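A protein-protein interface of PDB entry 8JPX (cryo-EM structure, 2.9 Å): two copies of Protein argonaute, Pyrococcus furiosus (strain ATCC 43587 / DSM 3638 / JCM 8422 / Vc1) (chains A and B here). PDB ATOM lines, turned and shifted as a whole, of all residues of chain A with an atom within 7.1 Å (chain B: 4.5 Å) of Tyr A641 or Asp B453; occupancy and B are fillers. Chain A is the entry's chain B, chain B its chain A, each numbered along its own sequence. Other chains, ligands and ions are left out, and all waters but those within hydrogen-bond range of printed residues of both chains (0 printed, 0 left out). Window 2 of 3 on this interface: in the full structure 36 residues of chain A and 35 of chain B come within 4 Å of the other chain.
Among the printed residues, merely in contact across the chains: Gly A638 with Tyr B197 and Phe A646 with Ile B457.
Printed residues of chain B within 4 Å of Lys A605: Asp B453 (3.3 Å) and Glu B490 (3.3 Å).
Of the printed residues of chain B, Gly A638 touches Tyr B197.
Printed residues of chain A within 4 Å of Tyr B197: Gly A638 (3.3 Å).
Of the printed residues of chain A, Ile B457 touches Phe A646.
Printed residues of chain A within 4 Å of Glu B490: Lys A605 (3.3 Å).
The nearest residue of chain B that does not touch Tyr A641 is Tyr B197 (4.03 Å).
The side-chain carboxylate (OD2) of Asp B453 is in hydrogen-bond range of the side-chain amide nitrogen (ND2) of Asn A601.
The side-chain carboxylate of Asp B453 is in salt-bridge range of the side-chain amino group of Lys A605 (3.3 Å).
OE1 of Glu B490 is in salt-bridge range of NZ of Lys A605 (3.8 Å).
OH of Tyr A641 is in hydrogen-bond range of OD2 of Asp B453.
No position is printed for both chains.
Of the 6 pairs that touch across the chains among the printed residues, none has its exchanged pair printed and touching as well.
Hydrophobic or aromatic side chains of chain A within 4 Å of the printed part of chain B: Tyr A641 and Phe A646.
Along chain A the printed residues that touch a printed residue of chain B span positions 601 to 646.
Of the 9 printed residues of chain B, 4 touch a printed residue of chain A.
Printed residues of chain B that touch a printed residue of chain A: Tyr B197, Asp B453, Ile B457 and Glu B490.
Hydrophobic or aromatic side chains of chain B that line the printed part of chain A: Tyr B197 and Ile B457.
Among the printed residues, 6 pairs touch across the chains.
Among the printed residues, Asp or Glu carboxylates within 4 Å of a Lys or Arg side-chain nitrogen of the other chain: Lys A605 with Asp B453 and Lys A605 with Glu B490.
The side-chain sulfur (SD) of Met A645 lies close to the side-chain hydroxyl (OH) of Tyr A641, at 3.7 Å.
The side-chain amino group (NZ) of Lys B487 lies within salt-bridge range of the side-chain carboxylate (OD1) of Asp B453 (3.3 Å).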
ATOM      1  N   ASN A 601      13.489  13.598  18.877  1.00  0.00           N
ATOM      2  CA  ASN A 601      14.423  13.476  17.764  1.00  0.00           C
ATOM      3  C   ASN A 601      15.090  14.811  17.456  1.00  0.00           C
ATOM      4  O   ASN A 601      16.300  14.865  17.219  1.00  0.00           O
ATOM      5  CB  ASN A 601      13.703  12.937  16.531  1.00  0.00           C
ATOM      6  CG  ASN A 601      14.647  12.276  15.549  1.00  0.00           C
ATOM      7  OD1 ASN A 601      15.752  11.875  15.909  1.00  0.00           O
ATOM      8  ND2 ASN A 601      14.216  12.160  14.300  1.00  0.00           N
ATOM      9  N   LYS A 605      19.274  16.195  18.138  1.00  0.00           N
ATOM     10  CA  LYS A 605      19.993  16.794  17.021  1.00  0.00           C
ATOM     11  C   LYS A 605      20.496  18.185  17.381  1.00  0.00           C
ATOM     12  O   LYS A 605      21.628  18.553  17.046  1.00  0.00           O
ATOM     13  CB  LYS A 605      19.095  16.846  15.786  1.00  0.00           C
ATOM     14  CG  LYS A 605      18.885  15.496  15.123  1.00  0.00           C
ATOM     15  CD  LYS A 605      18.628  15.645  13.634  1.00  0.00           C
ATOM     16  CE  LYS A 605      17.182  16.014  13.363  1.00  0.00           C
ATOM     17  NZ  LYS A 605      16.297  14.819  13.372  1.00  0.00           N
ATOM     18  N   GLU A 636       8.432   8.722  24.998  1.00  0.00           N
ATOM     19  CA  GLU A 636       9.082   7.449  25.286  1.00  0.00           C
ATOM     20  C   GLU A 636       9.355   6.668  24.008  1.00  0.00           C
ATOM     21  O   GLU A 636      10.408   6.036  23.872  1.00  0.00           O
ATOM     22  CB  GLU A 636       8.224   6.627  26.244  1.00  0.00           C
ATOM     23  CG  GLU A 636       8.748   5.227  26.495  1.00  0.00           C
ATOM     24  CD  GLU A 636       7.655   4.183  26.440  1.00  0.00           C
ATOM     25  OE1 GLU A 636       6.718   4.346  25.631  1.00  0.00           O
ATOM     26  OE2 GLU A 636       7.731   3.198  27.204  1.00  0.00           O
ATOM     27  N   GLU A 637       8.417   6.698  23.061  1.00  0.00           N
ATOM     28  CA  GLU A 637       8.616   6.000  21.796  1.00  0.00           C
ATOM     29  C   GLU A 637       9.743   6.623  20.986  1.00  0.00           C
ATOM     30  O   GLU A 637      10.484   5.906  20.305  1.00  0.00           O
ATOM     31  CB  GLU A 637       7.314   5.998  20.995  1.00  0.00           C
ATOM     32  CG  GLU A 637       7.418   5.362  19.624  1.00  0.00           C
ATOM     33  CD  GLU A 637       6.221   5.672  18.750  1.00  0.00           C
ATOM     34  OE1 GLU A 637       5.124   5.898  19.302  1.00  0.00           O
ATOM     35  OE2 GLU A 637       6.375   5.690  17.511  1.00  0.00           O
ATOM     36  N   GLY A 638       9.893   7.943  21.047  1.00  0.00           N
ATOM     37  CA  GLY A 638      10.971   8.607  20.342  1.00  0.00           C
ATOM     38  C   GLY A 638      12.316   8.553  21.028  1.00  0.00           C
ATOM     39  O   GLY A 638      13.315   8.956  20.428  1.00  0.00           O
ATOM     40  N   LEU A 639      12.370   8.068  22.268  1.00  0.00           N
ATOM     41  CA  LEU A 639      13.650   7.908  22.947  1.00  0.00           C
ATOM     42  C   LEU A 639      14.322   6.593  22.578  1.00  0.00           C
ATOM     43  O   LEU A 639      15.556   6.526  22.522  1.00  0.00           O
ATOM     44  CB  LEU A 639      13.458   7.996  24.461  1.00  0.00           C
ATOM     45  CG  LEU A 639      13.520   9.395  25.072  1.00  0.00           C
ATOM     46  CD1 LEU A 639      13.080   9.365  26.524  1.00  0.00           C
ATOM     47  CD2 LEU A 639      14.918   9.972  24.947  1.00  0.00           C
ATOM     48  N   LYS A 640      13.535   5.546  22.324  1.00  0.00           N
ATOM     49  CA  LYS A 640      14.101   4.288  21.854  1.00  0.00           C
ATOM     50  C   LYS A 640      14.747   4.458  20.486  1.00  0.00           C
ATOM     51  O   LYS A 640      15.800   3.872  20.208  1.00  0.00           O
ATOM     52  CB  LYS A 640      13.016   3.214  21.810  1.00  0.00           C
ATOM     53  CG  LYS A 640      12.307   3.016  23.135  1.00  0.00           C
ATOM     54  CD  LYS A 640      10.923   2.410  22.967  1.00  0.00           C
ATOM     55  CE  LYS A 640      10.872   1.423  21.817  1.00  0.00           C
ATOM     56  NZ  LYS A 640       9.509   0.853  21.646  1.00  0.00           N
ATOM     57  N   TYR A 641      14.130   5.262  19.619  1.00  0.00           N
ATOM     58  CA  TYR A 641      14.705   5.522  18.305  1.00  0.00           C
ATOM     59  C   TYR A 641      16.069   6.190  18.424  1.00  0.00           C
ATOM     60  O   TYR A 641      17.012   5.823  17.715  1.00  0.00           O
ATOM     61  CB  TYR A 641      13.746   6.385  17.489  1.00  0.00           C
ATOM     62  CG  TYR A 641      14.252   6.762  16.118  1.00  0.00           C
ATOM     63  CD1 TYR A 641      14.278   5.831  15.089  1.00  0.00           C
ATOM     64  CD2 TYR A 641      14.692   8.048  15.849  1.00  0.00           C
ATOM     65  CE1 TYR A 641      14.734   6.172  13.834  1.00  0.00           C
ATOM     66  CE2 TYR A 641      15.151   8.397  14.598  1.00  0.00           C
ATOM     67  CZ  TYR A 641      15.170   7.455  13.594  1.00  0.00           C
ATOM     68  OH  TYR A 641      15.626   7.798  12.344  1.00  0.00           O
ATOM     69  N   ILE A 642      16.194   7.174  19.317  1.00  0.00           N
ATOM     70  CA  ILE A 642      17.483   7.827  19.535  1.00  0.00           C
ATOM     71  C   ILE A 642      18.486   6.850  20.133  1.00  0.00           C
ATOM     72  O   ILE A 642      19.652   6.809  19.721  1.00  0.00           O
ATOM     73  CB  ILE A 642      17.310   9.080  20.414  1.00  0.00           C
ATOM     74  CG1 ILE A 642      17.033  10.312  19.550  1.00  0.00           C
ATOM     75  CG2 ILE A 642      18.532   9.309  21.290  1.00  0.00           C
ATOM     76  CD1 ILE A 642      15.705  10.301  18.854  1.00  0.00           C
ATOM     77  N   SER A 643      18.054   6.045  21.107  1.00  0.00           N
ATOM     78  CA  SER A 643      18.965   5.095  21.737  1.00  0.00           C
ATOM     79  C   SER A 643      19.466   4.055  20.746  1.00  0.00           C
ATOM     80  O   SER A 643      20.567   3.518  20.913  1.00  0.00           O
ATOM     81  CB  SER A 643      18.276   4.413  22.916  1.00  0.00           C
ATOM     82  OG  SER A 643      17.716   3.175  22.524  1.00  0.00           O
ATOM     83  N   GLU A 644      18.671   3.748  19.718  1.00  0.00           N
ATOM     84  CA  GLU A 644      19.111   2.796  18.702  1.00  0.00           C
ATOM     85  C   GLU A 644      20.329   3.308  17.944  1.00  0.00           C
ATOM     86  O   GLU A 644      21.267   2.549  17.678  1.00  0.00           O
ATOM     87  CB  GLU A 644      17.968   2.499  17.733  1.00  0.00           C
ATOM     88  CG  GLU A 644      17.239   1.199  18.012  1.00  0.00           C
ATOM     89  CD  GLU A 644      16.141   0.923  17.005  1.00  0.00           C
ATOM     90  OE1 GLU A 644      15.259   1.790  16.834  1.00  0.00           O
ATOM     91  OE2 GLU A 644      16.157  -0.162  16.387  1.00  0.00           O
ATOM     92  N   MET A 645      20.335   4.592  17.585  1.00  0.00           N
ATOM     93  CA  MET A 645      21.390   5.146  16.741  1.00  0.00           C
ATOM     94  C   MET A 645      22.564   5.689  17.554  1.00  0.00           C
ATOM     95  O   MET A 645      23.701   5.238  17.390  1.00  0.00           O
ATOM     96  CB  MET A 645      20.818   6.249  15.846  1.00  0.00           C
ATOM     97  CG  MET A 645      19.362   6.056  15.469  1.00  0.00           C
ATOM     98  SD  MET A 645      18.811   7.236  14.222  1.00  0.00           S
ATOM     99  CE  MET A 645      19.743   8.690  14.694  1.00  0.00           C
ATOM    100  N   PHE A 646      22.300   6.656  18.433  1.00  0.00           N
ATOM    101  CA  PHE A 646      23.368   7.393  19.097  1.00  0.00           C
ATOM    102  C   PHE A 646      24.153   6.560  20.101  1.00  0.00           C
ATOM    103  O   PHE A 646      25.224   7.001  20.530  1.00  0.00           O
ATOM    104  CB  PHE A 646      22.795   8.625  19.794  1.00  0.00           C
ATOM    105  CG  PHE A 646      22.650   9.814  18.892  1.00  0.00           C
ATOM    106  CD1 PHE A 646      23.766  10.436  18.362  1.00  0.00           C
ATOM    107  CD2 PHE A 646      21.398  10.308  18.573  1.00  0.00           C
ATOM    108  CE1 PHE A 646      23.635  11.529  17.532  1.00  0.00           C
ATOM    109  CE2 PHE A 646      21.261  11.401  17.742  1.00  0.00           C
ATOM    110  CZ  PHE A 646      22.381  12.012  17.221  1.00  0.00           C
ATOM    111  N   ILE A 702      16.298   3.274  29.268  1.00  0.00           N
ATOM    112  CA  ILE A 702      16.185   3.048  27.834  1.00  0.00           C
ATOM    113  C   ILE A 702      17.587   2.882  27.271  1.00  0.00           C
ATOM    114  O   ILE A 702      18.450   3.751  27.469  1.00  0.00           O
ATOM    115  CB  ILE A 702      15.448   4.198  27.131  1.00  0.00           C
ATOM    116  CG1 ILE A 702      14.113   4.472  27.819  1.00  0.00           C
ATOM    117  CG2 ILE A 702      15.235   3.870  25.666  1.00  0.00           C
ATOM    118  CD1 ILE A 702      13.482   5.776  27.416  1.00  0.00           C
ATOM    119  N   GLY A 705      17.368   0.602  22.119  1.00  0.00           N
ATOM    120  CA  GLY A 705      15.994   0.552  21.665  1.00  0.00           C
ATOM    121  C   GLY A 705      15.060  -0.237  22.549  1.00  0.00           C
ATOM    122  O   GLY A 705      13.983  -0.631  22.097  1.00  0.00           O
ATOM    123  N   TYR B 197       8.690   7.797  12.540  1.00  0.00           N
ATOM    124  CA  TYR B 197      10.023   7.233  12.346  1.00  0.00           C
ATOM    125  C   TYR B 197      10.015   6.074  11.356  1.00  0.00           C
ATOM    126  O   TYR B 197      10.631   6.159  10.289  1.00  0.00           O
ATOM    127  CB  TYR B 197      10.621   6.784  13.683  1.00  0.00           C
ATOM    128  CG  TYR B 197      10.461   7.796  14.793  1.00  0.00           C
ATOM    129  CD1 TYR B 197      10.957   9.084  14.661  1.00  0.00           C
ATOM    130  CD2 TYR B 197       9.809   7.463  15.972  1.00  0.00           C
ATOM    131  CE1 TYR B 197      10.812  10.012  15.670  1.00  0.00           C
ATOM    132  CE2 TYR B 197       9.659   8.385  16.987  1.00  0.00           C
ATOM    133  CZ  TYR B 197      10.161   9.658  16.831  1.00  0.00           C
ATOM    134  OH  TYR B 197      10.016  10.580  17.840  1.00  0.00           O
ATOM    135  N   SER B 452      18.608  10.526   5.200  1.00  0.00           N
ATOM    136  CA  SER B 452      18.517   9.863   6.490  1.00  0.00           C
ATOM    137  C   SER B 452      19.133  10.744   7.566  1.00  0.00           C
ATOM    138  O   SER B 452      19.960  11.615   7.289  1.00  0.00           O
ATOM    139  CB  SER B 452      19.212   8.496   6.469  1.00  0.00           C
ATOM    140  OG  SER B 452      20.585   8.619   6.791  1.00  0.00           O
ATOM    141  N   ASP B 453      18.710  10.506   8.810  1.00  0.00           N
ATOM    142  CA  ASP B 453      19.199  11.306   9.929  1.00  0.00           C
ATOM    143  C   ASP B 453      20.691  11.098  10.159  1.00  0.00           C
ATOM    144  O   ASP B 453      21.411  12.050  10.485  1.00  0.00           O
ATOM    145  CB  ASP B 453      18.411  10.970  11.194  1.00  0.00           C
ATOM    146  CG  ASP B 453      17.087  11.702  11.266  1.00  0.00           C
ATOM    147  OD1 ASP B 453      17.024  12.865  10.821  1.00  0.00           O
ATOM    148  OD2 ASP B 453      16.107  11.111  11.767  1.00  0.00           O
ATOM    149  N   LYS B 454      21.172   9.862  10.008  1.00  0.00           N
ATOM    150  CA  LYS B 454      22.584   9.580  10.251  1.00  0.00           C
ATOM    151  C   LYS B 454      23.478  10.340   9.278  1.00  0.00           C
ATOM    152  O   LYS B 454      24.506  10.904   9.676  1.00  0.00           O
ATOM    153  CB  LYS B 454      22.839   8.077  10.153  1.00  0.00           C
ATOM    154  CG  LYS B 454      22.246   7.274  11.297  1.00  0.00           C
ATOM    155  CD  LYS B 454      23.196   6.183  11.763  1.00  0.00           C
ATOM    156  CE  LYS B 454      24.373   6.766  12.525  1.00  0.00           C
ATOM    157  NZ  LYS B 454      23.975   7.933  13.359  1.00  0.00           N
ATOM    158  N   GLY B 455      23.103  10.364   7.998  1.00  0.00           N
ATOM    159  CA  GLY B 455      23.893  11.096   7.022  1.00  0.00           C
ATOM    160  C   GLY B 455      23.927  12.586   7.298  1.00  0.00           C
ATOM    161  O   GLY B 455      24.970  13.230   7.163  1.00  0.00           O
ATOM    162  N   ILE B 456      22.785  13.155   7.692  1.00  0.00           N
ATOM    163  CA  ILE B 456      22.734  14.577   8.015  1.00  0.00           C
ATOM    164  C   ILE B 456      23.601  14.877   9.230  1.00  0.00           C
ATOM    165  O   ILE B 456      24.315  15.888   9.268  1.00  0.00           O
ATOM    166  CB  ILE B 456      21.277  15.024   8.227  1.00  0.00           C
ATOM    167  CG1 ILE B 456      20.476  14.844   6.938  1.00  0.00           C
ATOM    168  CG2 ILE B 456      21.225  16.470   8.692  1.00  0.00           C
ATOM    169  CD1 ILE B 456      19.139  15.544   6.944  1.00  0.00           C
ATOM    170  N   ILE B 457      23.552  14.008  10.243  1.00  0.00           N
ATOM    171  CA  ILE B 457      24.384  14.198  11.428  1.00  0.00           C
ATOM    172  C   ILE B 457      25.860  14.166  11.053  1.00  0.00           C
ATOM    173  O   ILE B 457      26.650  15.002  11.507  1.00  0.00           O
ATOM    174  CB  ILE B 457      24.048  13.140  12.495  1.00  0.00           C
ATOM    175  CG1 ILE B 457      22.672  13.411  13.106  1.00  0.00           C
ATOM    176  CG2 ILE B 457      25.117  13.111  13.579  1.00  0.00           C
ATOM    177  CD1 ILE B 457      22.664  14.517  14.136  1.00  0.00           C
ATOM    178  N   LYS B 487      13.711  17.392   5.033  1.00  0.00           N
ATOM    179  CA  LYS B 487      15.123  17.048   4.929  1.00  0.00           C
ATOM    180  C   LYS B 487      15.912  18.103   4.169  1.00  0.00           C
ATOM    181  O   LYS B 487      17.038  18.427   4.554  1.00  0.00           O
ATOM    182  CB  LYS B 487      15.294  15.689   4.248  1.00  0.00           C
ATOM    183  CG  LYS B 487      14.735  14.532   5.049  1.00  0.00           C
ATOM    184  CD  LYS B 487      15.845  13.731   5.701  1.00  0.00           C
ATOM    185  CE  LYS B 487      15.295  12.813   6.775  1.00  0.00           C
ATOM    186  NZ  LYS B 487      15.210  13.505   8.089  1.00  0.00           N
ATOM    187  N   GLU B 490      15.808  20.847   6.691  1.00  0.00           N
ATOM    188  CA  GLU B 490      16.725  20.522   7.778  1.00  0.00           C
ATOM    189  C   GLU B 490      18.169  20.785   7.374  1.00  0.00           C
ATOM    190  O   GLU B 490      18.944  21.367   8.140  1.00  0.00           O
ATOM    191  CB  GLU B 490      16.545  19.065   8.201  1.00  0.00           C
ATOM    192  CG  GLU B 490      17.369  18.670   9.414  1.00  0.00           C
ATOM    193  CD  GLU B 490      16.837  17.429  10.099  1.00  0.00           C
ATOM    194  OE1 GLU B 490      15.724  17.488  10.660  1.00  0.00           O
ATOM    195  OE2 GLU B 490      17.534  16.393  10.075  1.00  0.00           O
